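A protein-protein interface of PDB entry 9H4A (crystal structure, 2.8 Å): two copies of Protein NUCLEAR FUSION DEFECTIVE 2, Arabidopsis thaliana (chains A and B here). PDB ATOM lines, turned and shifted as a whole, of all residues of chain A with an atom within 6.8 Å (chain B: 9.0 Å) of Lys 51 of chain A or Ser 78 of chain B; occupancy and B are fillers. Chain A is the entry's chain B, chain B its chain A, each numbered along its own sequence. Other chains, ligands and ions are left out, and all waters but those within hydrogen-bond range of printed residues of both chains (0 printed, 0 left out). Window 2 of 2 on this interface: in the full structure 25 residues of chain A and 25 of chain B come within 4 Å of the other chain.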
ATOM      1  N   ARG A  38     -24.996 -23.367 -27.588  1.00  0.00           N
ATOM      2  CA  ARG A  38     -25.215 -22.223 -26.712  1.00  0.00           C
ATOM      3  C   ARG A  38     -25.908 -21.084 -27.446  1.00  0.00           C
ATOM      4  O   ARG A  38     -26.638 -20.301 -26.827  1.00  0.00           O
ATOM      5  CB  ARG A  38     -23.884 -21.749 -26.131  1.00  0.00           C
ATOM      6  CG  ARG A  38     -24.007 -20.937 -24.858  1.00  0.00           C
ATOM      7  CD  ARG A  38     -22.717 -20.194 -24.559  1.00  0.00           C
ATOM      8  NE  ARG A  38     -22.721 -19.605 -23.224  1.00  0.00           N
ATOM      9  CZ  ARG A  38     -22.079 -20.122 -22.181  1.00  0.00           C
ATOM     10  NH1 ARG A  38     -21.375 -21.238 -22.319  1.00  0.00           N
ATOM     11  NH2 ARG A  38     -22.139 -19.523 -20.999  1.00  0.00           N
ATOM     12  N   THR A  41     -29.629 -21.773 -27.266  1.00  0.00           N
ATOM     13  CA  THR A  41     -30.195 -21.889 -25.929  1.00  0.00           C
ATOM     14  C   THR A  41     -30.650 -20.515 -25.451  1.00  0.00           C
ATOM     15  O   THR A  41     -29.827 -19.611 -25.268  1.00  0.00           O
ATOM     16  CB  THR A  41     -29.178 -22.488 -24.959  1.00  0.00           C
ATOM     17  OG1 THR A  41     -28.769 -23.777 -25.430  1.00  0.00           O
ATOM     18  CG2 THR A  41     -29.788 -22.633 -23.573  1.00  0.00           C
ATOM     19  N   HIS A  42     -31.956 -20.360 -25.253  1.00  0.00           N
ATOM     20  CA  HIS A  42     -32.505 -19.105 -24.766  1.00  0.00           C
ATOM     21  C   HIS A  42     -32.231 -18.949 -23.272  1.00  0.00           C
ATOM     22  O   HIS A  42     -31.902 -19.908 -22.569  1.00  0.00           O
ATOM     23  CB  HIS A  42     -34.009 -19.037 -25.047  1.00  0.00           C
ATOM     24  CG  HIS A  42     -34.628 -17.712 -24.729  1.00  0.00           C
ATOM     25  ND1 HIS A  42     -35.535 -17.540 -23.705  1.00  0.00           N
ATOM     26  CD2 HIS A  42     -34.465 -16.492 -25.296  1.00  0.00           C
ATOM     27  CE1 HIS A  42     -35.908 -16.274 -23.657  1.00  0.00           C
ATOM     28  NE2 HIS A  42     -35.273 -15.616 -24.610  1.00  0.00           N
ATOM     29  N   ALA A  43     -32.368 -17.710 -22.790  1.00  0.00           N
ATOM     30  CA  ALA A  43     -32.092 -17.421 -21.387  1.00  0.00           C
ATOM     31  C   ALA A  43     -33.067 -18.128 -20.454  1.00  0.00           C
ATOM     32  O   ALA A  43     -32.714 -18.429 -19.308  1.00  0.00           O
ATOM     33  CB  ALA A  43     -32.126 -15.912 -21.146  1.00  0.00           C
ATOM     34  N   ASN A  49     -26.557 -19.561 -21.806  1.00  0.00           N
ATOM     35  CA  ASN A  49     -27.473 -19.188 -22.880  1.00  0.00           C
ATOM     36  C   ASN A  49     -26.741 -18.270 -23.851  1.00  0.00           C
ATOM     37  O   ASN A  49     -25.508 -18.257 -23.926  1.00  0.00           O
ATOM     38  CB  ASN A  49     -28.742 -18.549 -22.301  1.00  0.00           C
ATOM     39  CG  ASN A  49     -28.441 -17.380 -21.389  1.00  0.00           C
ATOM     40  OD1 ASN A  49     -27.963 -16.339 -21.836  1.00  0.00           O
ATOM     41  ND2 ASN A  49     -28.716 -17.547 -20.100  1.00  0.00           N
ATOM     42  N   ASN A  50     -27.504 -17.485 -24.610  1.00  0.00           N
ATOM     43  CA  ASN A  50     -26.962 -16.728 -25.733  1.00  0.00           C
ATOM     44  C   ASN A  50     -27.156 -15.224 -25.582  1.00  0.00           C
ATOM     45  O   ASN A  50     -27.158 -14.501 -26.584  1.00  0.00           O
ATOM     46  CB  ASN A  50     -27.599 -17.204 -27.038  1.00  0.00           C
ATOM     47  CG  ASN A  50     -29.109 -17.145 -26.996  1.00  0.00           C
ATOM     48  OD1 ASN A  50     -29.694 -16.593 -26.064  1.00  0.00           O
ATOM     49  ND2 ASN A  50     -29.751 -17.715 -28.005  1.00  0.00           N
ATOM     50  N   LYS A  51     -27.333 -14.732 -24.353  1.00  0.00           N
ATOM     51  CA  LYS A  51     -27.495 -13.294 -24.164  1.00  0.00           C
ATOM     52  C   LYS A  51     -26.218 -12.542 -24.524  1.00  0.00           C
ATOM     53  O   LYS A  51     -26.274 -11.475 -25.144  1.00  0.00           O
ATOM     54  CB  LYS A  51     -27.909 -12.988 -22.725  1.00  0.00           C
ATOM     55  CG  LYS A  51     -29.360 -13.315 -22.413  1.00  0.00           C
ATOM     56  CD  LYS A  51     -29.889 -12.439 -21.286  1.00  0.00           C
ATOM     57  CE  LYS A  51     -29.060 -12.586 -20.019  1.00  0.00           C
ATOM     58  NZ  LYS A  51     -29.550 -11.693 -18.928  1.00  0.00           N
ATOM     59  N   ALA A  52     -25.059 -13.083 -24.146  1.00  0.00           N
ATOM     60  CA  ALA A  52     -23.801 -12.425 -24.482  1.00  0.00           C
ATOM     61  C   ALA A  52     -23.452 -12.600 -25.954  1.00  0.00           C
ATOM     62  O   ALA A  52     -22.859 -11.699 -26.559  1.00  0.00           O
ATOM     63  CB  ALA A  52     -22.675 -12.959 -23.598  1.00  0.00           C
ATOM     64  N   LEU A  53     -23.811 -13.742 -26.546  1.00  0.00           N
ATOM     65  CA  LEU A  53     -23.533 -13.959 -27.963  1.00  0.00           C
ATOM     66  C   LEU A  53     -24.411 -13.090 -28.854  1.00  0.00           C
ATOM     67  O   LEU A  53     -23.962 -12.650 -29.919  1.00  0.00           O
ATOM     68  CB  LEU A  53     -23.723 -15.435 -28.314  1.00  0.00           C
ATOM     69  CG  LEU A  53     -22.643 -16.395 -27.817  1.00  0.00           C
ATOM     70  CD1 LEU A  53     -23.015 -17.836 -28.130  1.00  0.00           C
ATOM     71  CD2 LEU A  53     -21.300 -16.037 -28.435  1.00  0.00           C
ATOM     72  N   SER A  54     -25.657 -12.834 -28.446  1.00  0.00           N
ATOM     73  CA  SER A  54     -26.542 -12.012 -29.267  1.00  0.00           C
ATOM     74  C   SER A  54     -26.085 -10.561 -29.302  1.00  0.00           C
ATOM     75  O   SER A  54     -26.244  -9.889 -30.326  1.00  0.00           O
ATOM     76  CB  SER A  54     -27.978 -12.102 -28.752  1.00  0.00           C
ATOM     77  OG  SER A  54     -28.120 -11.438 -27.508  1.00  0.00           O
ATOM     78  N   ILE A  55     -25.523 -10.063 -28.199  1.00  0.00           N
ATOM     79  CA  ILE A  55     -24.964  -8.714 -28.188  1.00  0.00           C
ATOM     80  C   ILE A  55     -23.803  -8.616 -29.168  1.00  0.00           C
ATOM     81  O   ILE A  55     -23.659  -7.622 -29.891  1.00  0.00           O
ATOM     82  CB  ILE A  55     -24.540  -8.327 -26.759  1.00  0.00           C
ATOM     83  CG1 ILE A  55     -25.765  -8.234 -25.846  1.00  0.00           C
ATOM     84  CG2 ILE A  55     -23.762  -7.019 -26.759  1.00  0.00           C
ATOM     85  CD1 ILE A  55     -25.444  -7.772 -24.442  1.00  0.00           C
ATOM     86  N   PHE A  56     -22.958  -9.649 -29.209  1.00  0.00           N
ATOM     87  CA  PHE A  56     -21.895  -9.705 -30.207  1.00  0.00           C
ATOM     88  C   PHE A  56     -22.477  -9.707 -31.616  1.00  0.00           C
ATOM     89  O   PHE A  56     -22.013  -8.970 -32.494  1.00  0.00           O
ATOM     90  CB  PHE A  56     -21.033 -10.947 -29.972  1.00  0.00           C
ATOM     91  CG  PHE A  56     -19.755 -10.977 -30.774  1.00  0.00           C
ATOM     92  CD1 PHE A  56     -19.285  -9.844 -31.418  1.00  0.00           C
ATOM     93  CD2 PHE A  56     -19.025 -12.150 -30.881  1.00  0.00           C
ATOM     94  CE1 PHE A  56     -18.114  -9.881 -32.153  1.00  0.00           C
ATOM     95  CE2 PHE A  56     -17.854 -12.192 -31.615  1.00  0.00           C
ATOM     96  CZ  PHE A  56     -17.399 -11.056 -32.251  1.00  0.00           C
ATOM     97  N   THR A 124     -33.021 -12.896 -31.046  1.00  0.00           N
ATOM     98  CA  THR A 124     -31.877 -13.165 -30.182  1.00  0.00           C
ATOM     99  C   THR A 124     -31.087 -14.368 -30.685  1.00  0.00           C
ATOM    100  O   THR A 124     -29.854 -14.320 -30.779  1.00  0.00           O
ATOM    101  CB  THR A 124     -32.346 -13.385 -28.743  1.00  0.00           C
ATOM    102  OG1 THR A 124     -32.989 -12.197 -28.264  1.00  0.00           O
ATOM    103  CG2 THR A 124     -31.168 -13.715 -27.841  1.00  0.00           C
ATOM    104  N   ALA A 128     -27.233 -14.383 -32.199  1.00  0.00           N
ATOM    105  CA  ALA A 128     -26.281 -15.254 -31.518  1.00  0.00           C
ATOM    106  C   ALA A 128     -25.578 -16.208 -32.475  1.00  0.00           C
ATOM    107  O   ALA A 128     -24.511 -16.732 -32.136  1.00  0.00           O
ATOM    108  CB  ALA A 128     -26.987 -16.046 -30.418  1.00  0.00           C
ATOM    109  N   LEU B  70     -15.152 -12.330 -25.381  1.00  0.00           N
ATOM    110  CA  LEU B  70     -15.902 -13.570 -25.540  1.00  0.00           C
ATOM    111  C   LEU B  70     -15.009 -14.748 -25.903  1.00  0.00           C
ATOM    112  O   LEU B  70     -15.403 -15.898 -25.680  1.00  0.00           O
ATOM    113  CB  LEU B  70     -16.994 -13.393 -26.595  1.00  0.00           C
ATOM    114  CG  LEU B  70     -18.321 -12.820 -26.099  1.00  0.00           C
ATOM    115  CD1 LEU B  70     -19.207 -12.435 -27.267  1.00  0.00           C
ATOM    116  CD2 LEU B  70     -19.026 -13.826 -25.207  1.00  0.00           C
ATOM    117  N   ASP B  73     -13.392 -15.581 -22.117  1.00  0.00           N
ATOM    118  CA  ASP B  73     -14.417 -16.057 -21.189  1.00  0.00           C
ATOM    119  C   ASP B  73     -15.742 -16.142 -21.941  1.00  0.00           C
ATOM    120  O   ASP B  73     -16.396 -15.120 -22.175  1.00  0.00           O
ATOM    121  CB  ASP B  73     -14.520 -15.135 -19.977  1.00  0.00           C
ATOM    122  CG  ASP B  73     -15.373 -15.720 -18.868  1.00  0.00           C
ATOM    123  OD1 ASP B  73     -15.699 -16.923 -18.937  1.00  0.00           O
ATOM    124  OD2 ASP B  73     -15.719 -14.973 -17.927  1.00  0.00           O
ATOM    125  N   ILE B  74     -16.138 -17.360 -22.319  1.00  0.00           N
ATOM    126  CA  ILE B  74     -17.423 -17.550 -22.980  1.00  0.00           C
ATOM    127  C   ILE B  74     -18.577 -17.407 -21.994  1.00  0.00           C
ATOM    128  O   ILE B  74     -19.702 -17.092 -22.400  1.00  0.00           O
ATOM    129  CB  ILE B  74     -17.458 -18.919 -23.689  1.00  0.00           C
ATOM    130  CG1 ILE B  74     -18.684 -19.034 -24.599  1.00  0.00           C
ATOM    131  CG2 ILE B  74     -17.433 -20.055 -22.675  1.00  0.00           C
ATOM    132  CD1 ILE B  74     -18.723 -18.007 -25.707  1.00  0.00           C
ATOM    133  N   ASP B  75     -18.323 -17.614 -20.699  1.00  0.00           N
ATOM    134  CA  ASP B  75     -19.345 -17.499 -19.666  1.00  0.00           C
ATOM    135  C   ASP B  75     -19.458 -16.086 -19.104  1.00  0.00           C
ATOM    136  O   ASP B  75     -19.891 -15.913 -17.957  1.00  0.00           O
ATOM    137  CB  ASP B  75     -19.067 -18.496 -18.539  1.00  0.00           C
ATOM    138  CG  ASP B  75     -19.198 -19.938 -18.989  1.00  0.00           C
ATOM    139  OD1 ASP B  75     -19.994 -20.205 -19.913  1.00  0.00           O
ATOM    140  OD2 ASP B  75     -18.508 -20.806 -18.414  1.00  0.00           O
ATOM    141  N   ILE B  76     -19.078 -15.072 -19.876  1.00  0.00           N
ATOM    142  CA  ILE B  76     -19.182 -13.691 -19.420  1.00  0.00           C
ATOM    143  C   ILE B  76     -20.639 -13.255 -19.475  1.00  0.00           C
ATOM    144  O   ILE B  76     -21.367 -13.571 -20.425  1.00  0.00           O
ATOM    145  CB  ILE B  76     -18.281 -12.770 -20.264  1.00  0.00           C
ATOM    146  CG1 ILE B  76     -18.377 -11.323 -19.772  1.00  0.00           C
ATOM    147  CG2 ILE B  76     -18.641 -12.855 -21.740  1.00  0.00           C
ATOM    148  CD1 ILE B  76     -17.532 -10.351 -20.566  1.00  0.00           C
ATOM    149  N   SER B  77     -21.080 -12.545 -18.442  1.00  0.00           N
ATOM    150  CA  SER B  77     -22.451 -12.060 -18.412  1.00  0.00           C
ATOM    151  C   SER B  77     -22.632 -10.930 -19.419  1.00  0.00           C
ATOM    152  O   SER B  77     -21.707 -10.166 -19.704  1.00  0.00           O
ATOM    153  CB  SER B  77     -22.825 -11.579 -17.010  1.00  0.00           C
ATOM    154  OG  SER B  77     -22.104 -10.411 -16.660  1.00  0.00           O
ATOM    155  N   SER B  78     -23.847 -10.837 -19.967  1.00  0.00           N
ATOM    156  CA  SER B  78     -24.140  -9.774 -20.922  1.00  0.00           C
ATOM    157  C   SER B  78     -24.020  -8.399 -20.277  1.00  0.00           C
ATOM    158  O   SER B  78     -23.691  -7.422 -20.959  1.00  0.00           O
ATOM    159  CB  SER B  78     -25.535  -9.969 -21.513  1.00  0.00           C
ATOM    160  OG  SER B  78     -26.527  -9.952 -20.502  1.00  0.00           O
ATOM    161  N   LYS B  79     -24.276  -8.305 -18.971  1.00  0.00           N
ATOM    162  CA  LYS B  79     -24.104  -7.034 -18.276  1.00  0.00           C
ATOM    163  C   LYS B  79     -22.634  -6.642 -18.203  1.00  0.00           C
ATOM    164  O   LYS B  79     -22.292  -5.462 -18.347  1.00  0.00           O
ATOM    165  CB  LYS B  79     -24.709  -7.117 -16.876  1.00  0.00           C
ATOM    166  CG  LYS B  79     -26.192  -7.450 -16.862  1.00  0.00           C
ATOM    167  CD  LYS B  79     -26.728  -7.516 -15.441  1.00  0.00           C
ATOM    168  CE  LYS B  79     -28.213  -7.847 -15.420  1.00  0.00           C
ATOM    169  NZ  LYS B  79     -28.741  -7.936 -14.030  1.00  0.00           N
ATOM    170  N   ALA B  80     -21.749  -7.616 -17.980  1.00  0.00           N
ATOM    171  CA  ALA B  80     -20.322  -7.319 -17.933  1.00  0.00           C
ATOM    172  C   ALA B  80     -19.792  -6.941 -19.310  1.00  0.00           C
ATOM    173  O   ALA B  80     -19.010  -5.993 -19.441  1.00  0.00           O
ATOM    174  CB  ALA B  80     -19.554  -8.513 -17.369  1.00  0.00           C
ATOM    175  N   LEU B  81     -20.209  -7.672 -20.348  1.00  0.00           N
ATOM    176  CA  LEU B  81     -19.761  -7.360 -21.701  1.00  0.00           C
ATOM    177  C   LEU B  81     -20.198  -5.963 -22.118  1.00  0.00           C
ATOM    178  O   LEU B  81     -19.463  -5.257 -22.819  1.00  0.00           O
ATOM    179  CB  LEU B  81     -20.295  -8.404 -22.683  1.00  0.00           C
ATOM    180  CG  LEU B  81     -19.837  -8.282 -24.137  1.00  0.00           C
ATOM    181  CD1 LEU B  81     -18.346  -8.554 -24.260  1.00  0.00           C
ATOM    182  CD2 LEU B  81     -20.633  -9.217 -25.035  1.00  0.00           C
ATOM    183  N   GLY B  82     -21.391  -5.543 -21.693  1.00  0.00           N
ATOM    184  CA  GLY B  82     -21.857  -4.210 -22.032  1.00  0.00           C
ATOM    185  C   GLY B  82     -21.056  -3.119 -21.348  1.00  0.00           C
ATOM    186  O   GLY B  82     -20.757  -2.085 -21.952  1.00  0.00           O
ATOM    187  N   ARG B  83     -20.699  -3.331 -20.079  1.00  0.00           N
ATOM    188  CA  ARG B  83     -19.878  -2.354 -19.371  1.00  0.00           C
ATOM    189  C   ARG B  83     -18.486  -2.259 -19.980  1.00  0.00           C
ATOM    190  O   ARG B  83     -17.917  -1.165 -20.072  1.00  0.00           O
ATOM    191  CB  ARG B  83     -19.795  -2.713 -17.887  1.00  0.00           C
ATOM    192  CG  ARG B  83     -20.998  -2.266 -17.069  1.00  0.00           C
ATOM    193  CD  ARG B  83     -21.016  -2.925 -15.696  1.00  0.00           C
ATOM    194  NE  ARG B  83     -19.797  -2.668 -14.935  1.00  0.00           N
ATOM    195  CZ  ARG B  83     -19.679  -1.725 -14.005  1.00  0.00           C
ATOM    196  NH1 ARG B  83     -20.710  -0.942 -13.718  1.00  0.00           N
ATOM    197  NH2 ARG B  83     -18.531  -1.565 -13.361  1.00  0.00           N
ATOM    198  N   LEU B  84     -17.924  -3.391 -20.410  1.00  0.00           N
ATOM    199  CA  LEU B  84     -16.592  -3.369 -21.008  1.00  0.00           C
ATOM    200  C   LEU B  84     -16.599  -2.698 -22.376  1.00  0.00           C
ATOM    201  O   LEU B  84     -15.606  -2.071 -22.759  1.00  0.00           O
ATOM    202  CB  LEU B  84     -16.038  -4.790 -21.111  1.00  0.00           C
ATOM    203  CG  LEU B  84     -15.870  -5.538 -19.785  1.00  0.00           C
ATOM    204  CD1 LEU B  84     -15.249  -6.907 -20.011  1.00  0.00           C
ATOM    205  CD2 LEU B  84     -15.046  -4.721 -18.800  1.00  0.00           C
ATOM    206  N   ILE B  85     -17.698  -2.820 -23.123  1.00  0.00           N
ATOM    207  CA  ILE B  85     -17.804  -2.115 -24.397  1.00  0.00           C
ATOM    208  C   ILE B  85     -17.903  -0.613 -24.165  1.00  0.00           C
ATOM    209  O   ILE B  85     -17.308   0.185 -24.899  1.00  0.00           O
ATOM    210  CB  ILE B  85     -19.003  -2.645 -25.206  1.00  0.00           C
ATOM    211  CG1 ILE B  85     -18.736  -4.072 -25.687  1.00  0.00           C
ATOM    212  CG2 ILE B  85     -19.298  -1.740 -26.390  1.00  0.00           C
ATOM    213  CD1 ILE B  85     -19.892  -4.684 -26.448  1.00  0.00           C
ATOM    214  N   SER B  86     -18.642  -0.202 -23.130  1.00  0.00           N
ATOM    215  CA  SER B  86     -18.785   1.219 -22.841  1.00  0.00           C
ATOM    216  C   SER B  86     -17.490   1.828 -22.315  1.00  0.00           C
ATOM    217  O   SER B  86     -17.239   3.020 -22.525  1.00  0.00           O
ATOM    218  CB  SER B  86     -19.921   1.439 -21.840  1.00  0.00           C
ATOM    219  OG  SER B  86     -21.150   0.955 -22.352  1.00  0.00           O
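No position is printed for both chains. Of the 8 pairs that touch across the chains among the printed residues, none has its exchanged pair printed and touching as well.
The side-chain carboxylate of Asp 75 of chain B is in salt-bridge range of the guanidinium group of Arg 38 of chain A, 2.5 Å away.
Among the printed residues, pairs that only touch across the chains: Ala 52 of chain A with Ile 76 of chain B (3.5 Å), Phe 56 of chain A with Leu 70 of chain B (3.6 Å), Ile 55 of chain A with Ser 78 of chain B (3.7 Å), Ala 52 of chain A with Leu 81 of chain B (3.7 Å), Lys 51 of chain A with Ser 78 of chain B (3.7 Å), Arg 38 of chain A with Ile 74 of chain B (3.7 Å) and Ala 52 of chain A with Leu 70 of chain B (3.8 Å).
The guanidinium group of Arg 38 of chain A lies within hydrogen-bond range of the backbone carbonyl oxygen of Asn 49 of chain A, at 3.2 Å. OD1 of Asn 49 of chain A lies within hydrogen-bond range of N of Lys 51 of chain A (3.1 Å). The backbone carbonyl oxygen (O) of Lys 51 of chain A sits at hydrogen-bond distance from the side-chain hydroxyl (OG) of Ser 54 of chain A (3.0 Å). The side-chain carboxylate (OD1) of Asp 73 of chain B lies close to the backbone NH (N) of Asp 75 of chain B, at 3.2 Å.
Of chain B, only Ser 78 (3.7 Å) comes within 4 Å of Lys 51 of chain A. Ser 78 of chain B touches just these residues of chain A: Lys 51 (3.7 Å) and Ile 55 (3.7 Å). Of chain B, only Leu 70 (3.8 Å), Ile 76 (3.5 Å) and Leu 81 (3.7 Å) come within 4 Å of Ala 52 of chain A. Printed residues of chain B within 4 Å of Ile 55 of chain A: Ser 78 (3.7 Å). Of the printed residues of chain B, Phe 56 of chain A touches Leu 70 (3.6 Å). Of the printed residues of chain A, Ile 76 of chain B touches Ala 52. Ala 128 of chain A touches none of the printed residues of chain B.
Of the 15 printed residues of chain B, 6 touch a printed residue of chain A. Hydrophobic or aromatic side chains of chain B within 4 Å of the printed part of chain A: Leu 70 and Leu 81. Hydrophobic or aromatic side chains of chain A within 4 Å of the printed part of chain B: Ala 52, Ile 55 and Phe 56. Among the printed residues, Asp or Glu carboxylates within 4 Å of a Lys or Arg side-chain nitrogen of the other chain: Arg 38 of chain A with Asp 75 of chain B.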
